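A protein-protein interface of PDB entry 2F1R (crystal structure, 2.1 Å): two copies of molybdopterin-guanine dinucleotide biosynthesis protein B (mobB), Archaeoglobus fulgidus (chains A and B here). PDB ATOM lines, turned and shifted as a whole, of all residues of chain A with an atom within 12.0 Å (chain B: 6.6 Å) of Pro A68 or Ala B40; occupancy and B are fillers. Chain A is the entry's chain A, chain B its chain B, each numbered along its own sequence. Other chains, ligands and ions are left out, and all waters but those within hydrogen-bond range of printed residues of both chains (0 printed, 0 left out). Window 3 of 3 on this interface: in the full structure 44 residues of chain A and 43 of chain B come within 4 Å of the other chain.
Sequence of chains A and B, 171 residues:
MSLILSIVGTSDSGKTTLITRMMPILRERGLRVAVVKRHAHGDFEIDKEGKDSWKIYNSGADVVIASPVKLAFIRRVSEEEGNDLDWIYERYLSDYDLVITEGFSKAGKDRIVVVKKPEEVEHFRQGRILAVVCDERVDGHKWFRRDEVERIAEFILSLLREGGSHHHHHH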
ATOM      1  N   VAL A  64      -2.291  -4.203 -35.503  1.00  0.00           N
ATOM      2  CA  VAL A  64      -1.123  -3.974 -34.621  1.00  0.00           C
ATOM      3  C   VAL A  64      -1.337  -2.682 -33.863  1.00  0.00           C
ATOM      4  O   VAL A  64      -1.574  -1.644 -34.474  1.00  0.00           O
ATOM      5  CB  VAL A  64       0.251  -3.937 -35.371  1.00  0.00           C
ATOM      6  CG1 VAL A  64       1.382  -3.572 -34.432  1.00  0.00           C
ATOM      7  CG2 VAL A  64       0.592  -5.260 -35.991  1.00  0.00           C
ATOM      8  N   ILE A  65      -1.306  -2.758 -32.541  1.00  0.00           N
ATOM      9  CA  ILE A  65      -1.361  -1.572 -31.707  1.00  0.00           C
ATOM     10  C   ILE A  65       0.041  -1.329 -31.202  1.00  0.00           C
ATOM     11  O   ILE A  65       0.605  -2.157 -30.486  1.00  0.00           O
ATOM     12  CB  ILE A  65      -2.353  -1.721 -30.551  1.00  0.00           C
ATOM     13  CG1 ILE A  65      -3.687  -2.198 -31.103  1.00  0.00           C
ATOM     14  CG2 ILE A  65      -2.616  -0.372 -29.894  1.00  0.00           C
ATOM     15  CD1 ILE A  65      -4.787  -2.400 -30.049  1.00  0.00           C
ATOM     16  N   ALA A  66       0.632  -0.221 -31.656  1.00  0.00           N
ATOM     17  CA  ALA A  66       2.038   0.090 -31.399  1.00  0.00           C
ATOM     18  C   ALA A  66       2.130   1.235 -30.421  1.00  0.00           C
ATOM     19  O   ALA A  66       1.347   2.205 -30.467  1.00  0.00           O
ATOM     20  CB  ALA A  66       2.768   0.442 -32.702  1.00  0.00           C
ATOM     21  N   SER A  67       3.073   1.113 -29.510  1.00  0.00           N
ATOM     22  CA  SER A  67       3.341   2.165 -28.543  1.00  0.00           C
ATOM     23  C   SER A  67       4.808   2.105 -28.379  1.00  0.00           C
ATOM     24  O   SER A  67       5.429   1.160 -28.895  1.00  0.00           O
ATOM     25  CB  SER A  67       2.631   1.881 -27.237  1.00  0.00           C
ATOM     26  OG  SER A  67       3.431   1.132 -26.343  1.00  0.00           O
ATOM     27  N   PRO A  68       5.395   3.100 -27.666  1.00  0.00           N
ATOM     28  CA  PRO A  68       6.833   3.116 -27.541  1.00  0.00           C
ATOM     29  C   PRO A  68       7.410   1.934 -26.818  1.00  0.00           C
ATOM     30  O   PRO A  68       8.539   1.615 -27.071  1.00  0.00           O
ATOM     31  CB  PRO A  68       7.105   4.400 -26.721  1.00  0.00           C
ATOM     32  CG  PRO A  68       5.844   5.219 -26.912  1.00  0.00           C
ATOM     33  CD  PRO A  68       4.764   4.235 -26.959  1.00  0.00           C
ATOM     34  N   VAL A  69       6.708   1.320 -25.870  1.00  0.00           N
ATOM     35  CA  VAL A  69       7.314   0.186 -25.196  1.00  0.00           C
ATOM     36  C   VAL A  69       6.508  -1.140 -25.215  1.00  0.00           C
ATOM     37  O   VAL A  69       6.941  -2.164 -24.625  1.00  0.00           O
ATOM     38  CB  VAL A  69       7.861   0.521 -23.787  1.00  0.00           C
ATOM     39  CG1 VAL A  69       9.289   1.266 -23.895  1.00  0.00           C
ATOM     40  CG2 VAL A  69       6.788   1.257 -22.917  1.00  0.00           C
ATOM     41  N   LYS A  70       5.373  -1.128 -25.922  1.00  0.00           N
ATOM     42  CA  LYS A  70       4.482  -2.273 -25.913  1.00  0.00           C
ATOM     43  C   LYS A  70       3.826  -2.399 -27.280  1.00  0.00           C
ATOM     44  O   LYS A  70       3.425  -1.402 -27.867  1.00  0.00           O
ATOM     45  CB  LYS A  70       3.421  -2.064 -24.825  1.00  0.00           C
ATOM     46  CG  LYS A  70       2.505  -3.257 -24.582  1.00  0.00           C
ATOM     47  CD  LYS A  70       1.160  -2.809 -24.063  1.00  0.00           C
ATOM     48  CE  LYS A  70       1.130  -2.695 -22.574  1.00  0.00           C
ATOM     49  NZ  LYS A  70      -0.123  -2.011 -22.111  1.00  0.00           N
ATOM     50  N   LEU A  71       3.695  -3.597 -27.770  1.00  0.00           N
ATOM     51  CA  LEU A  71       3.027  -3.880 -29.042  1.00  0.00           C
ATOM     52  C   LEU A  71       2.063  -5.056 -28.904  1.00  0.00           C
ATOM     53  O   LEU A  71       2.401  -6.054 -28.217  1.00  0.00           O
ATOM     54  CB  LEU A  71       4.069  -4.169 -30.127  1.00  0.00           C
ATOM     55  CG  LEU A  71       3.573  -4.142 -31.573  1.00  0.00           C
ATOM     56  CD1 LEU A  71       4.608  -3.496 -32.481  1.00  0.00           C
ATOM     57  CD2 LEU A  71       3.243  -5.548 -32.053  1.00  0.00           C
ATOM     58  N   ALA A  72       0.882  -4.944 -29.467  1.00  0.00           N
ATOM     59  CA  ALA A  72      -0.139  -5.993 -29.442  1.00  0.00           C
ATOM     60  C   ALA A  72      -0.447  -6.287 -30.883  1.00  0.00           C
ATOM     61  O   ALA A  72      -0.659  -5.349 -31.656  1.00  0.00           O
ATOM     62  CB  ALA A  72      -1.405  -5.521 -28.700  1.00  0.00           C
ATOM     63  N   ARG B  38      -0.708   3.392 -34.069  1.00  0.00           N
ATOM     64  CA  ARG B  38       0.200   3.866 -33.045  1.00  0.00           C
ATOM     65  C   ARG B  38      -0.462   4.699 -31.904  1.00  0.00           C
ATOM     66  O   ARG B  38      -1.209   5.653 -32.155  1.00  0.00           O
ATOM     67  CB  ARG B  38       1.330   4.649 -33.723  1.00  0.00           C
ATOM     68  CG  ARG B  38       2.287   5.281 -32.774  1.00  0.00           C
ATOM     69  CD  ARG B  38       3.563   5.558 -33.478  1.00  0.00           C
ATOM     70  NE  ARG B  38       4.545   6.040 -32.532  1.00  0.00           N
ATOM     71  CZ  ARG B  38       4.860   7.316 -32.362  1.00  0.00           C
ATOM     72  NH1 ARG B  38       4.248   8.254 -33.075  1.00  0.00           N
ATOM     73  NH2 ARG B  38       5.772   7.638 -31.462  1.00  0.00           N
ATOM     74  N   HIS B  39      -0.183   4.298 -30.657  1.00  0.00           N
ATOM     75  CA  HIS B  39      -0.363   5.147 -29.458  1.00  0.00           C
ATOM     76  C   HIS B  39       1.001   5.660 -28.964  1.00  0.00           C
ATOM     77  O   HIS B  39       1.765   4.909 -28.379  1.00  0.00           O
ATOM     78  CB  HIS B  39      -1.059   4.372 -28.340  1.00  0.00           C
ATOM     79  CG  HIS B  39      -2.473   3.998 -28.656  1.00  0.00           C
ATOM     80  ND1 HIS B  39      -3.554   4.588 -28.037  1.00  0.00           N
ATOM     81  CD2 HIS B  39      -2.986   3.111 -29.542  1.00  0.00           C
ATOM     82  CE1 HIS B  39      -4.673   4.063 -28.510  1.00  0.00           C
ATOM     83  NE2 HIS B  39      -4.356   3.164 -29.425  1.00  0.00           N
ATOM     84  N   ALA B  40       1.265   6.957 -29.180  1.00  0.00           N
ATOM     85  CA  ALA B  40       2.584   7.602 -28.998  1.00  0.00           C
ATOM     86  C   ALA B  40       3.185   7.642 -27.569  1.00  0.00           C
ATOM     87  O   ALA B  40       2.474   7.531 -26.552  1.00  0.00           O
ATOM     88  CB  ALA B  40       2.542   9.008 -29.607  1.00  0.00           C
ATOM     89  N   VAL B  77       8.619  -3.900 -26.122  1.00  0.00           N
ATOM     90  CA  VAL B  77       9.532  -3.520 -27.165  1.00  0.00           C
ATOM     91  C   VAL B  77      10.411  -2.375 -26.624  1.00  0.00           C
ATOM     92  O   VAL B  77       9.977  -1.607 -25.749  1.00  0.00           O
ATOM     93  CB  VAL B  77       8.796  -3.111 -28.505  1.00  0.00           C
ATOM     94  CG1 VAL B  77       7.965  -4.279 -29.046  1.00  0.00           C
ATOM     95  CG2 VAL B  77       7.953  -1.900 -28.351  1.00  0.00           C
ATOM     96  N   SER B  78      11.616  -2.233 -27.143  1.00  0.00           N
ATOM     97  CA  SER B  78      12.385  -1.045 -26.843  1.00  0.00           C
ATOM     98  C   SER B  78      11.758   0.128 -27.585  1.00  0.00           C
ATOM     99  O   SER B  78      11.014  -0.077 -28.539  1.00  0.00           O
ATOM    100  CB  SER B  78      13.866  -1.236 -27.270  1.00  0.00           C
ATOM    101  OG  SER B  78      13.956  -1.219 -28.669  1.00  0.00           O
ATOM    102  N   GLU B  79      12.071   1.352 -27.184  1.00  0.00           N
ATOM    103  CA  GLU B  79      11.614   2.549 -27.889  1.00  0.00           C
ATOM    104  C   GLU B  79      11.933   2.567 -29.360  1.00  0.00           C
ATOM    105  O   GLU B  79      11.151   3.027 -30.198  1.00  0.00           O
ATOM    106  CB  GLU B  79      12.372   3.731 -27.347  1.00  0.00           C
ATOM    107  CG  GLU B  79      12.021   4.112 -25.976  1.00  0.00           C
ATOM    108  CD  GLU B  79      12.584   5.468 -25.663  1.00  0.00           C
ATOM    109  OE1 GLU B  79      11.966   6.180 -24.848  1.00  0.00           O
ATOM    110  OE2 GLU B  79      13.632   5.821 -26.257  1.00  0.00           O
ATOM    111  N   GLU B  80      13.149   2.133 -29.643  1.00  0.00           N
ATOM    112  CA  GLU B  80      13.681   2.100 -31.001  1.00  0.00           C
ATOM    113  C   GLU B  80      12.917   1.085 -31.833  1.00  0.00           C
ATOM    114  O   GLU B  80      12.639   1.366 -32.977  1.00  0.00           O
ATOM    115  CB  GLU B  80      15.193   1.843 -31.016  1.00  0.00           C
ATOM    116  CG  GLU B  80      16.041   2.924 -30.286  1.00  0.00           C
ATOM    117  CD  GLU B  80      16.078   2.780 -28.728  1.00  0.00           C
ATOM    118  OE1 GLU B  80      15.587   1.773 -28.145  1.00  0.00           O
ATOM    119  OE2 GLU B  80      16.630   3.693 -28.064  1.00  0.00           O
ATOM    120  N   GLU B  81      12.532  -0.058 -31.264  1.00  0.00           N
ATOM    121  CA  GLU B  81      11.679  -1.034 -31.999  1.00  0.00           C
ATOM    122  C   GLU B  81      10.257  -0.522 -32.172  1.00  0.00           C
ATOM    123  O   GLU B  81       9.730  -0.566 -33.274  1.00  0.00           O
ATOM    124  CB  GLU B  81      11.623  -2.373 -31.276  1.00  0.00           C
ATOM    125  CG  GLU B  81      12.955  -3.108 -31.323  1.00  0.00           C
ATOM    126  CD  GLU B  81      13.128  -4.137 -30.225  1.00  0.00           C
ATOM    127  OE1 GLU B  81      12.313  -4.211 -29.293  1.00  0.00           O
ATOM    128  OE2 GLU B  81      14.108  -4.890 -30.296  1.00  0.00           O
ATOM    129  N   GLY B  82       9.638  -0.054 -31.075  1.00  0.00           N
ATOM    130  CA  GLY B  82       8.231   0.374 -31.093  1.00  0.00           C
ATOM    131  C   GLY B  82       7.939   1.573 -32.011  1.00  0.00           C
ATOM    132  O   GLY B  82       6.842   1.661 -32.586  1.00  0.00           O
ATOM    133  N   ASN B  83       8.918   2.470 -32.171  1.00  0.00           N
ATOM    134  CA  ASN B  83       8.774   3.592 -33.075  1.00  0.00           C
ATOM    135  C   ASN B  83       9.230   3.340 -34.485  1.00  0.00           C
ATOM    136  O   ASN B  83       9.178   4.266 -35.298  1.00  0.00           O
ATOM    137  CB  ASN B  83       9.481   4.845 -32.537  1.00  0.00           C
ATOM    138  CG  ASN B  83       8.887   5.333 -31.218  1.00  0.00           C
ATOM    139  OD1 ASN B  83       9.619   5.639 -30.266  1.00  0.00           O
ATOM    140  ND2 ASN B  83       7.552   5.374 -31.135  1.00  0.00           N
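CG2 of Ile A65 touches CD2 of His B39, at 3.5 Å. O of Ala A66 touches CA of Arg B38, 3.3 Å away. His B39 touches Ser A67. Gly B82 touches Ser A67. His B39 touches Pro A68. Pro A68 touches Ala B40 (CG to C, 3.7 Å). O of Val B77 touches O of Pro A68, 3.8 Å away. CA of Glu B79 touches O of Pro A68, 3.3 Å away. Val B77 touches Lys A70 (CG2 to N, 3.6 Å).
OG of Ser A67 lies within hydrogen-bond range of O of Lys A70, at 3.0 Å. NH2 of Arg B38 sits close to ND2 of Asn B83, 2.9 Å away. The backbone NH (N) of Ser B78 lies within hydrogen-bond range of the side-chain carboxylate (OE1) of Glu B81, 3.0 Å away. The side-chain hydroxyl (OG) of Ser A67 sits close to the backbone NH (N) of Val A69 (3.3 Å). O of Glu B79 lies close to OD1 of Asn B83, 3.0 Å away. The backbone carbonyl oxygen (O) of Ala A72 sits at hydrogen-bond distance from the backbone NH (N) of Ile A65 (2.8 Å).
The backbone carbonyl oxygen of Ala A66 sits at hydrogen-bond distance from the backbone NH of His B39 (2.6 Å). The backbone carbonyl oxygen (O) of Val A69 is in hydrogen-bond range of the backbone NH (N) of Val B77 (2.8 Å). The backbone carbonyl oxygen (O) of Pro A68 sits close to the backbone carbonyl oxygen (O) of Ser B78.
Hydrophobic or aromatic side chains of chain A that line the printed part of chain B: Ile A65, Pro A68 and Val A69. Of the 10 printed residues of chain B, 7 touch a printed residue of chain A. Among the printed residues, no Asp or Glu carboxylate lies within 4 Å of a Lys or Arg side-chain nitrogen of the other chain.
No position is printed for both chains.
Val A64 touches none of the printed residues of chain B. Of the printed residues of chain B, Ile A65 touches His B39 (3.5 Å). Of the printed residues of chain B, Ser A67 touches His B39 (3.2 Å) and Gly B82 (3.6 Å). Pro A68 touches just these residues of chain B: His B39 (3.4 Å), Ala B40 (3.7 Å), Val B77 (3.8 Å), Ser B78 (3.3 Å) and Glu B79 (3.3 Å). Leu A71 touches none of the printed residues of chain B. Of chain A, only Ile A65, Ala A66, Ser A67 and Pro A68 come within 4 Å of His B39. Ala B40 touches just one residue of chain A: Pro A68 (3.7 Å). Of chain A, only Pro A68 (3.3 Å) comes within 4 Å of Ser B78. Of the printed residues of chain A, Glu B79 touches Pro A68. The nearest printed residue of chain B that does not touch Ala A66 is Gly B82 (4.3 Å).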
